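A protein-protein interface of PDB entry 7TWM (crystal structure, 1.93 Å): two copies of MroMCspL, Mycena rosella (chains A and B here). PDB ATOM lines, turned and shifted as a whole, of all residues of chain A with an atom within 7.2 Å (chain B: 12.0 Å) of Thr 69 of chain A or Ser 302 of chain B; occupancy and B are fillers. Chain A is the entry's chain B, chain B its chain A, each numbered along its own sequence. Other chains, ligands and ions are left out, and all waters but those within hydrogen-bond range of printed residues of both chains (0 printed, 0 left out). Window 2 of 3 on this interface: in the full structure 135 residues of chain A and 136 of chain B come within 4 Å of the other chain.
O of Tyr 67 of chain A is in hydrogen-bond range of NZ of Lys 305 of chain B.
The backbone NH (N) of Ser 302 of chain B sits at hydrogen-bond distance from the side-chain carboxylate (OD2) of Asp 68 of chain A (2.8 Å).
O of Val 393 of chain B sits at hydrogen-bond distance from OH of Tyr 67 of chain A.
The backbone carbonyl oxygen of Asp 68 of chain A lies within hydrogen-bond range of the guanidinium group of Arg 73 of chain A (2.9 Å).
O of Lys 71 of chain A is in hydrogen-bond range of NH2 of Arg 73 of chain A (3.3 Å).
Among the printed residues, merely in contact across the chains: Tyr 67 of chain A with Phe 299 of chain B, Tyr 67 of chain A with Leu 392 of chain B, Asp 68 of chain A with Phe 299 of chain B, Asp 68 of chain A with Pro 301 of chain B, Thr 69 of chain A with Ser 302 of chain B and Lys 71 of chain A with Phe 299 of chain B.
Of chain B, only Ser 302 comes within 4 Å of Thr 69 of chain A.
Of chain A, only Asp 68 (2.8 Å) and Thr 69 (3.8 Å) come within 4 Å of Ser 302 of chain B.
No residue of chain B comes within 4 Å of Met 182 of chain A.
Of the printed residues of chain B, Lys 71 of chain A touches Phe 299 (3.5 Å).
Of the printed residues of chain A, Pro 301 of chain B touches Asp 68.
Of the printed residues of chain A, Phe 299 of chain B touches Tyr 67 (3.98 Å), Asp 68 (3.5 Å) and Lys 71 (3.5 Å).
Of the printed residues of chain A, Lys 305 of chain B touches Tyr 67 (2.8 Å).
Leu 368 of chain B touches none of the printed residues of chain A.
The nearest residue of chain B that does not touch Thr 69 of chain A is Lys 305 of chain B (6.3 Å).
The nearest residue of chain A that does not touch Ser 302 of chain B is Asn 70 of chain A (4.7 Å).
Printed residues of chain B that touch a printed residue of chain A: Phe 299, Pro 301, Ser 302, Lys 305, Leu 392 and Val 393.
Along chain B the printed residues that touch a printed residue of chain A span positions 299 to 393.
Printed residues of chain A that touch a printed residue of chain B: Tyr 67, Asp 68, Thr 69 and Lys 71.
Hydrophobic or aromatic side chains of chain A that line the printed part of chain B: Tyr 67.
Among the printed residues, no Asp or Glu carboxylate lies within 4 Å of a Lys or Arg side-chain nitrogen of the other chain.
No position is printed for both chains.
Of the 9 pairs that touch across the chains among the printed residues, none has its exchanged pair printed and touching as well.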
ATOM      1  N   TYR A  67       7.562 -16.935 -16.341  1.00  0.00           N
ATOM      2  CA  TYR A  67       7.340 -18.369 -16.201  1.00  0.00           C
ATOM      3  C   TYR A  67       8.552 -19.037 -15.559  1.00  0.00           C
ATOM      4  O   TYR A  67       9.674 -18.543 -15.650  1.00  0.00           O
ATOM      5  CB  TYR A  67       7.078 -19.061 -17.539  1.00  0.00           C
ATOM      6  CG  TYR A  67       5.749 -18.717 -18.158  1.00  0.00           C
ATOM      7  CD1 TYR A  67       4.586 -18.732 -17.401  1.00  0.00           C
ATOM      8  CD2 TYR A  67       5.650 -18.381 -19.501  1.00  0.00           C
ATOM      9  CE1 TYR A  67       3.358 -18.412 -17.959  1.00  0.00           C
ATOM     10  CE2 TYR A  67       4.430 -18.061 -20.074  1.00  0.00           C
ATOM     11  CZ  TYR A  67       3.281 -18.073 -19.301  1.00  0.00           C
ATOM     12  OH  TYR A  67       2.073 -17.757 -19.850  1.00  0.00           O
ATOM     13  N   ASP A  68       8.299 -20.186 -14.928  1.00  0.00           N
ATOM     14  CA  ASP A  68       9.327 -20.962 -14.256  1.00  0.00           C
ATOM     15  C   ASP A  68       8.657 -22.202 -13.677  1.00  0.00           C
ATOM     16  O   ASP A  68       7.485 -22.154 -13.303  1.00  0.00           O
ATOM     17  CB  ASP A  68      10.027 -20.133 -13.175  1.00  0.00           C
ATOM     18  CG  ASP A  68      11.397 -20.645 -12.765  1.00  0.00           C
ATOM     19  OD1 ASP A  68      11.817 -21.705 -13.279  1.00  0.00           O
ATOM     20  OD2 ASP A  68      12.034 -19.975 -11.928  1.00  0.00           O
ATOM     21  N   THR A  69       9.399 -23.314 -13.634  1.00  0.00           N
ATOM     22  CA  THR A  69       8.883 -24.510 -12.984  1.00  0.00           C
ATOM     23  C   THR A  69       8.954 -24.317 -11.471  1.00  0.00           C
ATOM     24  O   THR A  69       9.767 -23.531 -10.974  1.00  0.00           O
ATOM     25  CB  THR A  69       9.533 -25.795 -13.517  1.00  0.00           C
ATOM     26  OG1 THR A  69      10.947 -25.600 -13.573  1.00  0.00           O
ATOM     27  CG2 THR A  69       9.008 -26.210 -14.875  1.00  0.00           C
ATOM     28  N   ASN A  70       8.057 -25.022 -10.768  1.00  0.00           N
ATOM     29  CA  ASN A  70       7.851 -24.912  -9.330  1.00  0.00           C
ATOM     30  C   ASN A  70       7.078 -23.632  -9.018  1.00  0.00           C
ATOM     31  O   ASN A  70       6.498 -23.504  -7.941  1.00  0.00           O
ATOM     32  CB  ASN A  70       9.146 -25.054  -8.518  1.00  0.00           C
ATOM     33  CG  ASN A  70       9.906 -26.329  -8.821  1.00  0.00           C
ATOM     34  OD1 ASN A  70      11.084 -26.282  -9.166  1.00  0.00           O
ATOM     35  ND2 ASN A  70       9.243 -27.470  -8.711  1.00  0.00           N
ATOM     36  N   LYS A  71       7.074 -22.697  -9.976  1.00  0.00           N
ATOM     37  CA  LYS A  71       6.310 -21.466  -9.857  1.00  0.00           C
ATOM     38  C   LYS A  71       4.941 -21.678 -10.494  1.00  0.00           C
ATOM     39  O   LYS A  71       4.847 -22.133 -11.633  1.00  0.00           O
ATOM     40  CB  LYS A  71       7.070 -20.309 -10.509  1.00  0.00           C
ATOM     41  CG  LYS A  71       6.388 -18.954 -10.419  1.00  0.00           C
ATOM     42  CD  LYS A  71       7.225 -17.854 -11.019  1.00  0.00           C
ATOM     43  CE  LYS A  71       6.594 -16.486 -10.878  1.00  0.00           C
ATOM     44  NZ  LYS A  71       7.579 -15.421 -11.181  1.00  0.00           N
ATOM     45  N   LYS A  72       3.887 -21.358  -9.736  1.00  0.00           N
ATOM     46  CA  LYS A  72       2.525 -21.558 -10.206  1.00  0.00           C
ATOM     47  C   LYS A  72       2.179 -20.499 -11.254  1.00  0.00           C
ATOM     48  O   LYS A  72       2.618 -19.353 -11.164  1.00  0.00           O
ATOM     49  CB  LYS A  72       1.534 -21.662  -9.038  1.00  0.00           C
ATOM     50  CG  LYS A  72       1.458 -20.466  -8.098  1.00  0.00           C
ATOM     51  CD  LYS A  72       2.466 -20.502  -6.966  1.00  0.00           C
ATOM     52  CE  LYS A  72       2.119 -19.539  -5.851  1.00  0.00           C
ATOM     53  NZ  LYS A  72       3.227 -19.405  -4.875  1.00  0.00           N
ATOM     54  N   ARG A  73       1.403 -20.928 -12.255  1.00  0.00           N
ATOM     55  CA  ARG A  73       1.037 -20.127 -13.413  1.00  0.00           C
ATOM     56  C   ARG A  73       0.382 -18.816 -12.977  1.00  0.00           C
ATOM     57  O   ARG A  73       0.674 -17.754 -13.530  1.00  0.00           O
ATOM     58  CB  ARG A  73       0.134 -20.955 -14.333  1.00  0.00           C
ATOM     59  CG  ARG A  73       0.800 -21.445 -15.613  1.00  0.00           C
ATOM     60  CD  ARG A  73       2.102 -22.221 -15.502  1.00  0.00           C
ATOM     61  NE  ARG A  73       3.180 -21.403 -14.952  1.00  0.00           N
ATOM     62  CZ  ARG A  73       4.483 -21.571 -15.176  1.00  0.00           C
ATOM     63  NH1 ARG A  73       4.911 -22.541 -15.971  1.00  0.00           N
ATOM     64  NH2 ARG A  73       5.350 -20.750 -14.603  1.00  0.00           N
ATOM     65  N   THR A 181       1.084 -26.512 -16.179  1.00  0.00           N
ATOM     66  CA  THR A 181       2.466 -26.322 -15.759  1.00  0.00           C
ATOM     67  C   THR A 181       3.378 -26.270 -16.987  1.00  0.00           C
ATOM     68  O   THR A 181       3.362 -25.281 -17.721  1.00  0.00           O
ATOM     69  CB  THR A 181       2.871 -27.312 -14.658  1.00  0.00           C
ATOM     70  OG1 THR A 181       2.511 -28.636 -15.055  1.00  0.00           O
ATOM     71  CG2 THR A 181       2.242 -26.997 -13.317  1.00  0.00           C
ATOM     72  N   MET A 182       4.157 -27.339 -17.207  1.00  0.00           N
ATOM     73  CA  MET A 182       4.957 -27.479 -18.417  1.00  0.00           C
ATOM     74  C   MET A 182       5.205 -28.954 -18.735  1.00  0.00           C
ATOM     75  O   MET A 182       5.665 -29.279 -19.829  1.00  0.00           O
ATOM     76  CB  MET A 182       6.290 -26.726 -18.320  1.00  0.00           C
ATOM     77  CG  MET A 182       7.430 -27.541 -17.729  1.00  0.00           C
ATOM     78  SD  MET A 182       9.031 -27.179 -18.505  1.00  0.00           S
ATOM     79  CE  MET A 182       8.847 -28.024 -20.077  1.00  0.00           C
ATOM     80  N   VAL A 183       4.901 -29.838 -17.773  1.00  0.00           N
ATOM     81  CA  VAL A 183       5.040 -31.274 -17.971  1.00  0.00           C
ATOM     82  C   VAL A 183       3.931 -31.744 -18.915  1.00  0.00           C
ATOM     83  O   VAL A 183       2.985 -32.417 -18.507  1.00  0.00           O
ATOM     84  CB  VAL A 183       5.098 -32.050 -16.635  1.00  0.00           C
ATOM     85  CG1 VAL A 183       3.889 -31.808 -15.740  1.00  0.00           C
ATOM     86  CG2 VAL A 183       5.357 -33.538 -16.824  1.00  0.00           C
ATOM     87  N   ALA B 295       6.913  -9.986  -4.837  1.00  0.00           N
ATOM     88  CA  ALA B 295       8.000 -10.851  -5.278  1.00  0.00           C
ATOM     89  C   ALA B 295       8.488 -10.461  -6.676  1.00  0.00           C
ATOM     90  O   ALA B 295       9.554 -10.900  -7.108  1.00  0.00           O
ATOM     91  CB  ALA B 295       7.546 -12.291  -5.239  1.00  0.00           C
ATOM     92  N   SER B 298      12.130  -9.148  -7.598  1.00  0.00           N
ATOM     93  CA  SER B 298      13.236  -9.910  -7.031  1.00  0.00           C
ATOM     94  C   SER B 298      13.330 -11.313  -7.632  1.00  0.00           C
ATOM     95  O   SER B 298      14.346 -11.988  -7.453  1.00  0.00           O
ATOM     96  CB  SER B 298      13.112  -9.979  -5.526  1.00  0.00           C
ATOM     97  OG  SER B 298      12.039 -10.836  -5.151  1.00  0.00           O
ATOM     98  N   PHE B 299      12.262 -11.746  -8.319  1.00  0.00           N
ATOM     99  CA  PHE B 299      12.174 -13.078  -8.903  1.00  0.00           C
ATOM    100  C   PHE B 299      13.429 -13.386  -9.719  1.00  0.00           C
ATOM    101  O   PHE B 299      13.817 -12.609 -10.588  1.00  0.00           O
ATOM    102  CB  PHE B 299      10.903 -13.220  -9.748  1.00  0.00           C
ATOM    103  CG  PHE B 299      10.861 -14.432 -10.649  1.00  0.00           C
ATOM    104  CD1 PHE B 299      10.915 -15.720 -10.123  1.00  0.00           C
ATOM    105  CD2 PHE B 299      10.764 -14.290 -12.028  1.00  0.00           C
ATOM    106  CE1 PHE B 299      10.881 -16.832 -10.954  1.00  0.00           C
ATOM    107  CE2 PHE B 299      10.724 -15.404 -12.858  1.00  0.00           C
ATOM    108  CZ  PHE B 299      10.790 -16.673 -12.322  1.00  0.00           C
ATOM    109  N   VAL B 300      14.066 -14.525  -9.417  1.00  0.00           N
ATOM    110  CA  VAL B 300      15.175 -15.008 -10.226  1.00  0.00           C
ATOM    111  C   VAL B 300      14.881 -16.443 -10.673  1.00  0.00           C
ATOM    112  O   VAL B 300      14.714 -17.336  -9.838  1.00  0.00           O
ATOM    113  CB  VAL B 300      16.540 -14.838  -9.523  1.00  0.00           C
ATOM    114  CG1 VAL B 300      16.693 -15.709  -8.282  1.00  0.00           C
ATOM    115  CG2 VAL B 300      17.710 -15.036 -10.478  1.00  0.00           C
ATOM    116  N   PRO B 301      14.787 -16.697 -12.006  1.00  0.00           N
ATOM    117  CA  PRO B 301      14.423 -18.017 -12.535  1.00  0.00           C
ATOM    118  C   PRO B 301      15.352 -19.147 -12.099  1.00  0.00           C
ATOM    119  O   PRO B 301      16.531 -18.923 -11.839  1.00  0.00           O
ATOM    120  CB  PRO B 301      14.515 -17.851 -14.061  1.00  0.00           C
ATOM    121  CG  PRO B 301      14.372 -16.359 -14.290  1.00  0.00           C
ATOM    122  CD  PRO B 301      15.003 -15.707 -13.077  1.00  0.00           C
ATOM    123  N   SER B 302      14.788 -20.362 -12.039  1.00  0.00           N
ATOM    124  CA  SER B 302      15.482 -21.589 -11.673  1.00  0.00           C
ATOM    125  C   SER B 302      16.658 -21.839 -12.610  1.00  0.00           C
ATOM    126  O   SER B 302      17.646 -22.468 -12.228  1.00  0.00           O
ATOM    127  CB  SER B 302      14.542 -22.770 -11.723  1.00  0.00           C
ATOM    128  OG  SER B 302      13.483 -22.617 -10.793  1.00  0.00           O
ATOM    129  N   GLN B 303      16.511 -21.363 -13.849  1.00  0.00           N
ATOM    130  CA  GLN B 303      17.422 -21.705 -14.924  1.00  0.00           C
ATOM    131  C   GLN B 303      17.499 -20.532 -15.894  1.00  0.00           C
ATOM    132  O   GLN B 303      16.536 -19.787 -16.056  1.00  0.00           O
ATOM    133  CB  GLN B 303      16.925 -22.957 -15.643  1.00  0.00           C
ATOM    134  CG  GLN B 303      18.040 -23.768 -16.283  1.00  0.00           C
ATOM    135  CD  GLN B 303      17.516 -24.830 -17.219  1.00  0.00           C
ATOM    136  OE1 GLN B 303      18.272 -25.443 -17.972  1.00  0.00           O
ATOM    137  NE2 GLN B 303      16.212 -25.053 -17.186  1.00  0.00           N
ATOM    138  N   GLU B 304      18.670 -20.382 -16.517  1.00  0.00           N
ATOM    139  CA  GLU B 304      18.904 -19.341 -17.499  1.00  0.00           C
ATOM    140  C   GLU B 304      17.923 -19.514 -18.656  1.00  0.00           C
ATOM    141  O   GLU B 304      17.755 -20.611 -19.184  1.00  0.00           O
ATOM    142  CB  GLU B 304      20.346 -19.426 -17.993  1.00  0.00           C
ATOM    143  CG  GLU B 304      20.875 -18.096 -18.480  1.00  0.00           C
ATOM    144  CD  GLU B 304      22.185 -18.201 -19.235  1.00  0.00           C
ATOM    145  OE1 GLU B 304      22.681 -19.338 -19.421  1.00  0.00           O
ATOM    146  OE2 GLU B 304      22.699 -17.147 -19.641  1.00  0.00           O
ATOM    147  N   LYS B 305      17.270 -18.411 -19.020  1.00  0.00           N
ATOM    148  CA  LYS B 305      16.377 -18.387 -20.165  1.00  0.00           C
ATOM    149  C   LYS B 305      17.145 -17.874 -21.383  1.00  0.00           C
ATOM    150  O   LYS B 305      17.955 -16.961 -21.258  1.00  0.00           O
ATOM    151  CB  LYS B 305      15.155 -17.529 -19.826  1.00  0.00           C
ATOM    152  CG  LYS B 305      14.259 -18.131 -18.749  1.00  0.00           C
ATOM    153  CD  LYS B 305      13.040 -17.293 -18.417  1.00  0.00           C
ATOM    154  CE  LYS B 305      12.196 -17.882 -17.306  1.00  0.00           C
ATOM    155  NZ  LYS B 305      11.491 -19.105 -17.759  1.00  0.00           N
ATOM    156  N   ALA B 306      16.904 -18.501 -22.542  1.00  0.00           N
ATOM    157  CA  ALA B 306      17.405 -18.028 -23.826  1.00  0.00           C
ATOM    158  C   ALA B 306      16.756 -16.689 -24.163  1.00  0.00           C
ATOM    159  O   ALA B 306      15.639 -16.418 -23.731  1.00  0.00           O
ATOM    160  CB  ALA B 306      17.117 -19.056 -24.888  1.00  0.00           C
ATOM    161  N   LEU B 368      21.305 -18.672 -25.003  1.00  0.00           N
ATOM    162  CA  LEU B 368      21.519 -18.323 -23.605  1.00  0.00           C
ATOM    163  C   LEU B 368      22.478 -17.139 -23.525  1.00  0.00           C
ATOM    164  O   LEU B 368      23.496 -17.115 -24.216  1.00  0.00           O
ATOM    165  CB  LEU B 368      22.094 -19.532 -22.856  1.00  0.00           C
ATOM    166  CG  LEU B 368      21.199 -20.771 -22.768  1.00  0.00           C
ATOM    167  CD1 LEU B 368      21.932 -21.919 -22.076  1.00  0.00           C
ATOM    168  CD2 LEU B 368      19.900 -20.458 -22.035  1.00  0.00           C
ATOM    169  N   PRO B 369      22.173 -16.105 -22.710  1.00  0.00           N
ATOM    170  CA  PRO B 369      23.082 -14.973 -22.528  1.00  0.00           C
ATOM    171  C   PRO B 369      24.507 -15.369 -22.148  1.00  0.00           C
ATOM    172  O   PRO B 369      25.456 -14.685 -22.524  1.00  0.00           O
ATOM    173  CB  PRO B 369      22.406 -14.153 -21.420  1.00  0.00           C
ATOM    174  CG  PRO B 369      20.935 -14.459 -21.605  1.00  0.00           C
ATOM    175  CD  PRO B 369      20.901 -15.924 -21.990  1.00  0.00           C
ATOM    176  N   SER B 370      24.645 -16.487 -21.426  1.00  0.00           N
ATOM    177  CA  SER B 370      25.950 -16.965 -20.995  1.00  0.00           C
ATOM    178  C   SER B 370      26.757 -17.452 -22.199  1.00  0.00           C
ATOM    179  O   SER B 370      27.962 -17.227 -22.258  1.00  0.00           O
ATOM    180  CB  SER B 370      25.835 -18.015 -19.914  1.00  0.00           C
ATOM    181  OG  SER B 370      25.255 -19.214 -20.412  1.00  0.00           O
ATOM    182  N   ALA B 391       5.789 -23.687 -27.679  1.00  0.00           N
ATOM    183  CA  ALA B 391       4.555 -23.019 -27.271  1.00  0.00           C
ATOM    184  C   ALA B 391       4.418 -22.834 -25.756  1.00  0.00           C
ATOM    185  O   ALA B 391       5.100 -23.490 -24.972  1.00  0.00           O
ATOM    186  CB  ALA B 391       3.343 -23.684 -27.884  1.00  0.00           C
ATOM    187  N   LEU B 392       3.510 -21.917 -25.378  1.00  0.00           N
ATOM    188  CA  LEU B 392       3.247 -21.498 -24.006  1.00  0.00           C
ATOM    189  C   LEU B 392       1.746 -21.257 -23.829  1.00  0.00           C
ATOM    190  O   LEU B 392       1.143 -20.523 -24.612  1.00  0.00           O
ATOM    191  CB  LEU B 392       4.018 -20.202 -23.710  1.00  0.00           C
ATOM    192  CG  LEU B 392       5.480 -20.144 -24.155  1.00  0.00           C
ATOM    193  CD1 LEU B 392       5.621 -19.343 -25.442  1.00  0.00           C
ATOM    194  CD2 LEU B 392       6.351 -19.535 -23.066  1.00  0.00           C
ATOM    195  N   VAL B 393       1.159 -21.857 -22.779  1.00  0.00           N
ATOM    196  CA  VAL B 393      -0.269 -21.743 -22.497  1.00  0.00           C
ATOM    197  C   VAL B 393      -0.504 -20.682 -21.423  1.00  0.00           C
ATOM    198  O   VAL B 393       0.251 -20.598 -20.458  1.00  0.00           O
ATOM    199  CB  VAL B 393      -0.907 -23.091 -22.098  1.00  0.00           C
ATOM    200  CG1 VAL B 393      -1.525 -23.821 -23.284  1.00  0.00           C
ATOM    201  CG2 VAL B 393       0.052 -23.992 -21.332  1.00  0.00           C
